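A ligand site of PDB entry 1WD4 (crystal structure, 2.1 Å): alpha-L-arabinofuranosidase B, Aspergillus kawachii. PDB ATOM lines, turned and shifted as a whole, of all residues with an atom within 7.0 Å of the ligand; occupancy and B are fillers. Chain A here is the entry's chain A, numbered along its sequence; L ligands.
An oxygen (O3) of the ligand is in hydrogen-bond range of the side-chain carboxylate (OD2) of Asp 202.
O4 of the ligand lies within hydrogen-bond range of N of Asp 280, at 2.9 Å.
The side-chain carboxylate (OD2) of Asp 280 is in hydrogen-bond range of an oxygen (O5) of the ligand (2.6 Å).
The backbone NH (N) of Asn 205 sits at hydrogen-bond distance from an oxygen (O1) of the ligand (2.8 Å).
O1 of the ligand is in hydrogen-bond range of N of Asn 206, at 2.8 Å.
The backbone carbonyl oxygen (O) of Asn 206 lies within hydrogen-bond range of an oxygen (O1) of the ligand, at 3.4 Å.
OE1 of Glu 204 is in hydrogen-bond range of O4 of the ligand.
An oxygen (O3) of the ligand is in hydrogen-bond range of the backbone NH (N) of Gly 279 (3.2 Å).
The side-chain sulfur (SD) of Met 178 sits at hydrogen-bond distance from an oxygen (O3) of the ligand, at 3.6 Å.
Residues that only touch the ligand: Cys 159 (3.7 Å), Cys 160 (3.9 Å), Asp 162 (3.96 Å), Trp 189 (3.5 Å), Leu 207 (3.9 Å) and Gly 278 (3.3 Å).
Hydrophobic or aromatic side chains within 4 Å of the ligand: Met 178, Trp 189 and Leu 207.
Within 4 Å of the ligand: Cys 159, Cys 160, Asp 162, Met 178, Trp 189, Asp 202, Glu 204, Asn 205, Asn 206, Leu 207, Gly 278, Gly 279 and Asp 280.
The side-chain carboxylate (OD2) of Asp 162 lies close to the side-chain carboxylate (OD2) of Asp 202 (2.6 Å).
The backbone carbonyl oxygen (O) of Asn 205 is in hydrogen-bond range of the side-chain hydroxyl (OH) of Tyr 264, at 3.4 Å.
The side-chain amide oxygen (OD1) of Asn 206 sits at hydrogen-bond distance from the side-chain hydroxyl (OH) of Tyr 264 (3.2 Å).
The side-chain carboxylate (OE2) of Glu 167 lies close to the side-chain carboxylate (OE1) of Glu 204.
The side-chain sulfur (SD) of Met 178 lies close to the backbone NH (N) of Gly 279 (3.6 Å).
SG of Cys 160 forms a disulfide with SG of Cys 159.
SG of Cys 159 sits close to OG of Ser 282, at 3.7 Å.
The backbone NH of Ile 277 lies close to the backbone carbonyl oxygen of Cys 160 (3.2 Å).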
ATOM      1  N   PHE A  92     -20.464   0.023   9.798  1.00  0.00           N
ATOM      2  CA  PHE A  92     -20.699  -1.140   8.941  1.00  0.00           C
ATOM      3  C   PHE A  92     -20.383  -0.743   7.505  1.00  0.00           C
ATOM      4  O   PHE A  92     -20.585   0.410   7.117  1.00  0.00           O
ATOM      5  CB  PHE A  92     -22.160  -1.592   9.015  1.00  0.00           C
ATOM      6  CG  PHE A  92     -22.527  -2.261  10.315  1.00  0.00           C
ATOM      7  CD1 PHE A  92     -22.139  -3.563  10.570  1.00  0.00           C
ATOM      8  CD2 PHE A  92     -23.262  -1.576  11.273  1.00  0.00           C
ATOM      9  CE1 PHE A  92     -22.476  -4.186  11.770  1.00  0.00           C
ATOM     10  CE2 PHE A  92     -23.599  -2.180  12.479  1.00  0.00           C
ATOM     11  CZ  PHE A  92     -23.201  -3.491  12.731  1.00  0.00           C
ATOM     12  N   CYS A 159     -32.003  -3.327  10.746  1.00  0.00           N
ATOM     13  CA  CYS A 159     -31.591  -1.943  10.972  1.00  0.00           C
ATOM     14  C   CYS A 159     -30.954  -1.337   9.727  1.00  0.00           C
ATOM     15  O   CYS A 159     -30.038  -1.939   9.159  1.00  0.00           O
ATOM     16  CB  CYS A 159     -30.593  -1.893  12.119  1.00  0.00           C
ATOM     17  SG  CYS A 159     -30.133  -0.203  12.598  1.00  0.00           S
ATOM     18  N   CYS A 160     -31.425  -0.175   9.286  1.00  0.00           N
ATOM     19  CA  CYS A 160     -32.544   0.573   9.871  1.00  0.00           C
ATOM     20  C   CYS A 160     -33.037   1.482   8.750  1.00  0.00           C
ATOM     21  O   CYS A 160     -32.232   2.159   8.113  1.00  0.00           O
ATOM     22  CB  CYS A 160     -32.077   1.474  11.020  1.00  0.00           C
ATOM     23  SG  CYS A 160     -31.929   0.738  12.682  1.00  0.00           S
ATOM     24  N   ASP A 162     -34.133   4.633   8.067  1.00  0.00           N
ATOM     25  CA  ASP A 162     -34.247   5.960   8.659  1.00  0.00           C
ATOM     26  C   ASP A 162     -34.208   7.121   7.652  1.00  0.00           C
ATOM     27  O   ASP A 162     -33.813   6.971   6.493  1.00  0.00           O
ATOM     28  CB  ASP A 162     -33.091   6.212   9.634  1.00  0.00           C
ATOM     29  CG  ASP A 162     -33.151   5.333  10.865  1.00  0.00           C
ATOM     30  OD1 ASP A 162     -33.980   4.403  10.939  1.00  0.00           O
ATOM     31  OD2 ASP A 162     -32.334   5.592  11.786  1.00  0.00           O
ATOM     32  N   GLU A 167     -25.145  10.924  12.989  1.00  0.00           N
ATOM     33  CA  GLU A 167     -23.736  11.236  13.226  1.00  0.00           C
ATOM     34  C   GLU A 167     -22.993  11.632  11.952  1.00  0.00           C
ATOM     35  O   GLU A 167     -23.209  11.042  10.880  1.00  0.00           O
ATOM     36  CB  GLU A 167     -23.008  10.043  13.870  1.00  0.00           C
ATOM     37  CG  GLU A 167     -23.505   9.699  15.259  1.00  0.00           C
ATOM     38  CD  GLU A 167     -24.457   8.537  15.263  1.00  0.00           C
ATOM     39  OE1 GLU A 167     -25.194   8.346  14.271  1.00  0.00           O
ATOM     40  OE2 GLU A 167     -24.477   7.806  16.281  1.00  0.00           O
ATOM     41  N   SER A 170     -20.564   8.681  10.602  1.00  0.00           N
ATOM     42  CA  SER A 170     -21.134   7.424  10.144  1.00  0.00           C
ATOM     43  C   SER A 170     -20.864   6.287  11.141  1.00  0.00           C
ATOM     44  O   SER A 170     -20.848   5.113  10.770  1.00  0.00           O
ATOM     45  CB  SER A 170     -20.559   7.036   8.769  1.00  0.00           C
ATOM     46  OG  SER A 170     -20.788   8.067   7.809  1.00  0.00           O
ATOM     47  N   THR A 171     -20.656   6.654  12.401  1.00  0.00           N
ATOM     48  CA  THR A 171     -20.430   5.667  13.449  1.00  0.00           C
ATOM     49  C   THR A 171     -21.378   5.918  14.605  1.00  0.00           C
ATOM     50  O   THR A 171     -21.909   7.020  14.766  1.00  0.00           O
ATOM     51  CB  THR A 171     -18.981   5.727  13.991  1.00  0.00           C
ATOM     52  OG1 THR A 171     -18.692   7.046  14.458  1.00  0.00           O
ATOM     53  CG2 THR A 171     -17.991   5.325  12.911  1.00  0.00           C
ATOM     54  N   ASP A 172     -21.597   4.884  15.410  1.00  0.00           N
ATOM     55  CA  ASP A 172     -22.480   4.946  16.565  1.00  0.00           C
ATOM     56  C   ASP A 172     -21.707   5.626  17.705  1.00  0.00           C
ATOM     57  O   ASP A 172     -20.964   4.968  18.427  1.00  0.00           O
ATOM     58  CB  ASP A 172     -22.892   3.525  16.972  1.00  0.00           C
ATOM     59  CG  ASP A 172     -23.685   3.481  18.261  1.00  0.00           C
ATOM     60  OD1 ASP A 172     -23.863   4.534  18.906  1.00  0.00           O
ATOM     61  OD2 ASP A 172     -24.124   2.366  18.635  1.00  0.00           O
ATOM     62  N   THR A 173     -21.893   6.933  17.856  1.00  0.00           N
ATOM     63  CA  THR A 173     -21.189   7.654  18.903  1.00  0.00           C
ATOM     64  C   THR A 173     -21.966   7.753  20.209  1.00  0.00           C
ATOM     65  O   THR A 173     -21.631   8.557  21.070  1.00  0.00           O
ATOM     66  CB  THR A 173     -20.776   9.069  18.452  1.00  0.00           C
ATOM     67  OG1 THR A 173     -21.936   9.781  17.998  1.00  0.00           O
ATOM     68  CG2 THR A 173     -19.743   8.988  17.335  1.00  0.00           C
ATOM     69  N   MET A 178     -28.457  10.840  17.559  1.00  0.00           N
ATOM     70  CA  MET A 178     -29.312  10.642  16.394  1.00  0.00           C
ATOM     71  C   MET A 178     -30.730  11.100  16.717  1.00  0.00           C
ATOM     72  O   MET A 178     -31.113  11.197  17.878  1.00  0.00           O
ATOM     73  CB  MET A 178     -29.398   9.169  15.993  1.00  0.00           C
ATOM     74  CG  MET A 178     -28.180   8.569  15.323  1.00  0.00           C
ATOM     75  SD  MET A 178     -28.578   6.920  14.700  1.00  0.00           S
ATOM     76  CE  MET A 178     -29.595   7.387  13.307  1.00  0.00           C
ATOM     77  N   TRP A 189     -35.077  -3.122  19.394  1.00  0.00           N
ATOM     78  CA  TRP A 189     -35.101  -2.062  20.403  1.00  0.00           C
ATOM     79  C   TRP A 189     -36.545  -1.820  20.800  1.00  0.00           C
ATOM     80  O   TRP A 189     -37.121  -2.563  21.586  1.00  0.00           O
ATOM     81  CB  TRP A 189     -34.492  -0.786  19.821  1.00  0.00           C
ATOM     82  CG  TRP A 189     -33.023  -0.908  19.540  1.00  0.00           C
ATOM     83  CD1 TRP A 189     -32.003  -0.764  20.445  1.00  0.00           C
ATOM     84  CD2 TRP A 189     -32.403  -1.198  18.283  1.00  0.00           C
ATOM     85  NE1 TRP A 189     -30.786  -0.956  19.820  1.00  0.00           N
ATOM     86  CE2 TRP A 189     -31.006  -1.215  18.491  1.00  0.00           C
ATOM     87  CE3 TRP A 189     -32.904  -1.449  16.997  1.00  0.00           C
ATOM     88  CZ2 TRP A 189     -30.100  -1.478  17.458  1.00  0.00           C
ATOM     89  CZ3 TRP A 189     -31.998  -1.702  15.967  1.00  0.00           C
ATOM     90  CH2 TRP A 189     -30.611  -1.720  16.207  1.00  0.00           C
ATOM     91  N   VAL A 201     -38.759   6.694  16.438  1.00  0.00           N
ATOM     92  CA  VAL A 201     -37.722   7.711  16.374  1.00  0.00           C
ATOM     93  C   VAL A 201     -36.394   7.101  16.791  1.00  0.00           C
ATOM     94  O   VAL A 201     -36.242   6.618  17.906  1.00  0.00           O
ATOM     95  CB  VAL A 201     -38.059   8.909  17.290  1.00  0.00           C
ATOM     96  CG1 VAL A 201     -36.903   9.906  17.295  1.00  0.00           C
ATOM     97  CG2 VAL A 201     -39.318   9.584  16.812  1.00  0.00           C
ATOM     98  N   ASP A 202     -35.437   7.121  15.866  1.00  0.00           N
ATOM     99  CA  ASP A 202     -34.098   6.598  16.122  1.00  0.00           C
ATOM    100  C   ASP A 202     -33.298   7.684  16.852  1.00  0.00           C
ATOM    101  O   ASP A 202     -32.973   8.723  16.260  1.00  0.00           O
ATOM    102  CB  ASP A 202     -33.406   6.244  14.813  1.00  0.00           C
ATOM    103  CG  ASP A 202     -32.177   5.365  15.020  1.00  0.00           C
ATOM    104  OD1 ASP A 202     -31.548   5.460  16.094  1.00  0.00           O
ATOM    105  OD2 ASP A 202     -31.831   4.591  14.101  1.00  0.00           O
ATOM    106  N   MET A 203     -32.975   7.441  18.114  1.00  0.00           N
ATOM    107  CA  MET A 203     -32.203   8.406  18.887  1.00  0.00           C
ATOM    108  C   MET A 203     -30.793   7.857  19.166  1.00  0.00           C
ATOM    109  O   MET A 203     -30.062   8.396  20.003  1.00  0.00           O
ATOM    110  CB  MET A 203     -32.924   8.702  20.208  1.00  0.00           C
ATOM    111  CG  MET A 203     -34.251   9.449  20.039  1.00  0.00           C
ATOM    112  SD  MET A 203     -34.991   9.897  21.624  1.00  0.00           S
ATOM    113  CE  MET A 203     -36.733   9.803  21.279  1.00  0.00           C
ATOM    114  N   GLU A 204     -30.434   6.806  18.439  1.00  0.00           N
ATOM    115  CA  GLU A 204     -29.148   6.104  18.538  1.00  0.00           C
ATOM    116  C   GLU A 204     -29.174   5.115  19.689  1.00  0.00           C
ATOM    117  O   GLU A 204     -29.543   5.457  20.818  1.00  0.00           O
ATOM    118  CB  GLU A 204     -27.974   7.074  18.681  1.00  0.00           C
ATOM    119  CG  GLU A 204     -26.615   6.381  18.605  1.00  0.00           C
ATOM    120  CD  GLU A 204     -26.490   5.456  17.400  1.00  0.00           C
ATOM    121  OE1 GLU A 204     -25.981   5.876  16.344  1.00  0.00           O
ATOM    122  OE2 GLU A 204     -26.923   4.292  17.514  1.00  0.00           O
ATOM    123  N   ASN A 205     -28.778   3.872  19.403  1.00  0.00           N
ATOM    124  CA  ASN A 205     -28.788   2.784  20.383  1.00  0.00           C
ATOM    125  C   ASN A 205     -30.203   2.552  20.903  1.00  0.00           C
ATOM    126  O   ASN A 205     -30.383   2.113  22.041  1.00  0.00           O
ATOM    127  CB  ASN A 205     -27.887   3.094  21.566  1.00  0.00           C
ATOM    128  CG  ASN A 205     -26.445   2.826  21.276  1.00  0.00           C
ATOM    129  OD1 ASN A 205     -26.081   2.249  20.247  1.00  0.00           O
ATOM    130  ND2 ASN A 205     -25.601   3.238  22.187  1.00  0.00           N
ATOM    131  N   ASN A 206     -31.186   2.869  20.072  1.00  0.00           N
ATOM    132  CA  ASN A 206     -32.579   2.686  20.450  1.00  0.00           C
ATOM    133  C   ASN A 206     -33.526   3.291  19.433  1.00  0.00           C
ATOM    134  O   ASN A 206     -33.315   4.414  18.954  1.00  0.00           O
ATOM    135  CB  ASN A 206     -32.871   3.375  21.805  1.00  0.00           C
ATOM    136  CG  ASN A 206     -32.918   2.399  22.981  1.00  0.00           C
ATOM    137  OD1 ASN A 206     -32.497   2.754  24.080  1.00  0.00           O
ATOM    138  ND2 ASN A 206     -33.454   1.198  22.765  1.00  0.00           N
ATOM    139  N   LEU A 207     -34.551   2.522  19.085  1.00  0.00           N
ATOM    140  CA  LEU A 207     -35.597   2.984  18.197  1.00  0.00           C
ATOM    141  C   LEU A 207     -36.699   3.102  19.232  1.00  0.00           C
ATOM    142  O   LEU A 207     -36.978   2.140  19.946  1.00  0.00           O
ATOM    143  CB  LEU A 207     -35.942   1.931  17.135  1.00  0.00           C
ATOM    144  CG  LEU A 207     -34.845   1.654  16.099  1.00  0.00           C
ATOM    145  CD1 LEU A 207     -35.322   0.604  15.110  1.00  0.00           C
ATOM    146  CD2 LEU A 207     -34.484   2.941  15.370  1.00  0.00           C
ATOM    147  N   TYR A 264     -30.237  10.651  26.549  1.00  0.00           N
ATOM    148  CA  TYR A 264     -31.315  11.159  25.709  1.00  0.00           C
ATOM    149  C   TYR A 264     -31.816  12.561  26.080  1.00  0.00           C
ATOM    150  O   TYR A 264     -32.638  13.134  25.381  1.00  0.00           O
ATOM    151  CB  TYR A 264     -32.460  10.147  25.689  1.00  0.00           C
ATOM    152  CG  TYR A 264     -32.025   8.806  25.105  1.00  0.00           C
ATOM    153  CD1 TYR A 264     -31.599   8.727  23.771  1.00  0.00           C
ATOM    154  CD2 TYR A 264     -31.971   7.658  25.896  1.00  0.00           C
ATOM    155  CE1 TYR A 264     -31.129   7.516  23.244  1.00  0.00           C
ATOM    156  CE2 TYR A 264     -31.501   6.447  25.368  1.00  0.00           C
ATOM    157  CZ  TYR A 264     -31.076   6.384  24.050  1.00  0.00           C
ATOM    158  OH  TYR A 264     -30.577   5.199  23.542  1.00  0.00           O
ATOM    159  N   ILE A 274     -29.386  11.202   7.016  1.00  0.00           N
ATOM    160  CA  ILE A 274     -29.332   9.845   6.477  1.00  0.00           C
ATOM    161  C   ILE A 274     -30.662   9.456   5.886  1.00  0.00           C
ATOM    162  O   ILE A 274     -31.703   9.996   6.252  1.00  0.00           O
ATOM    163  CB  ILE A 274     -28.965   8.797   7.559  1.00  0.00           C
ATOM    164  CG1 ILE A 274     -29.959   8.882   8.731  1.00  0.00           C
ATOM    165  CG2 ILE A 274     -27.518   8.981   8.016  1.00  0.00           C
ATOM    166  CD1 ILE A 274     -29.762   7.821   9.806  1.00  0.00           C
ATOM    167  N   ILE A 277     -30.829   4.051   5.964  1.00  0.00           N
ATOM    168  CA  ILE A 277     -29.806   3.371   6.744  1.00  0.00           C
ATOM    169  C   ILE A 277     -29.774   3.849   8.188  1.00  0.00           C
ATOM    170  O   ILE A 277     -30.484   4.790   8.558  1.00  0.00           O
ATOM    171  CB  ILE A 277     -28.421   3.619   6.145  1.00  0.00           C
ATOM    172  CG1 ILE A 277     -28.235   5.132   5.947  1.00  0.00           C
ATOM    173  CG2 ILE A 277     -28.268   2.866   4.841  1.00  0.00           C
ATOM    174  CD1 ILE A 277     -26.856   5.550   5.470  1.00  0.00           C
ATOM    175  N   GLY A 278     -28.952   3.195   8.997  1.00  0.00           N
ATOM    176  CA  GLY A 278     -28.807   3.592  10.383  1.00  0.00           C
ATOM    177  C   GLY A 278     -27.633   4.557  10.514  1.00  0.00           C
ATOM    178  O   GLY A 278     -26.860   4.733   9.577  1.00  0.00           O
ATOM    179  N   GLY A 279     -27.500   5.189  11.673  1.00  0.00           N
ATOM    180  CA  GLY A 279     -26.417   6.147  11.875  1.00  0.00           C
ATOM    181  C   GLY A 279     -25.009   5.609  11.662  1.00  0.00           C
ATOM    182  O   GLY A 279     -24.137   6.321  11.175  1.00  0.00           O
ATOM    183  N   ASP A 280     -24.784   4.352  12.046  1.00  0.00           N
ATOM    184  CA  ASP A 280     -23.475   3.722  11.906  1.00  0.00           C
ATOM    185  C   ASP A 280     -23.373   3.002  10.560  1.00  0.00           C
ATOM    186  O   ASP A 280     -22.488   2.188  10.331  1.00  0.00           O
ATOM    187  CB  ASP A 280     -23.251   2.718  13.033  1.00  0.00           C
ATOM    188  CG  ASP A 280     -24.305   1.628  13.061  1.00  0.00           C
ATOM    189  OD1 ASP A 280     -25.178   1.605  12.157  1.00  0.00           O
ATOM    190  OD2 ASP A 280     -24.271   0.802  13.994  1.00  0.00           O
ATOM    191  N   ASN A 281     -24.326   3.337   9.683  1.00  0.00           N
ATOM    192  CA  ASN A 281     -24.468   2.776   8.347  1.00  0.00           C
ATOM    193  C   ASN A 281     -24.992   1.352   8.318  1.00  0.00           C
ATOM    194  O   ASN A 281     -24.656   0.580   7.422  1.00  0.00           O
ATOM    195  CB  ASN A 281     -23.174   2.834   7.523  1.00  0.00           C
ATOM    196  CG  ASN A 281     -23.440   2.553   6.038  1.00  0.00           C
ATOM    197  OD1 ASN A 281     -24.325   3.162   5.446  1.00  0.00           O
ATOM    198  ND2 ASN A 281     -22.695   1.605   5.445  1.00  0.00           N
ATOM    199  N   SER A 282     -25.791   0.975   9.312  1.00  0.00           N
ATOM    200  CA  SER A 282     -26.388  -0.359   9.293  1.00  0.00           C
ATOM    201  C   SER A 282     -27.206  -0.311   8.000  1.00  0.00           C
ATOM    202  O   SER A 282     -27.986   0.611   7.802  1.00  0.00           O
ATOM    203  CB  SER A 282     -27.305  -0.575  10.489  1.00  0.00           C
ATOM    204  OG  SER A 282     -26.562  -0.741  11.687  1.00  0.00           O
HETATM  205  O1  LIG L   1     -30.525   3.229  17.326  1.00  0.00           O
HETATM  206  C1  LIG L   1     -30.763   2.274  16.298  1.00  0.00           C
HETATM  207  C2  LIG L   1     -29.460   1.981  15.480  1.00  0.00           C
HETATM  208  O2  LIG L   1     -28.462   1.452  16.344  1.00  0.00           O
HETATM  209  C3  LIG L   1     -28.767   3.181  14.820  1.00  0.00           C
HETATM  210  O3  LIG L   1     -29.427   3.634  13.627  1.00  0.00           O
HETATM  211  C4  LIG L   1     -27.360   2.674  14.575  1.00  0.00           C
HETATM  212  O4  LIG L   1     -26.373   3.751  14.394  1.00  0.00           O
HETATM  213  C5  LIG L   1     -27.163   1.855  15.871  1.00  0.00           C
HETATM  214  O5  LIG L   1     -26.368   0.698  15.587  1.00  0.00           O
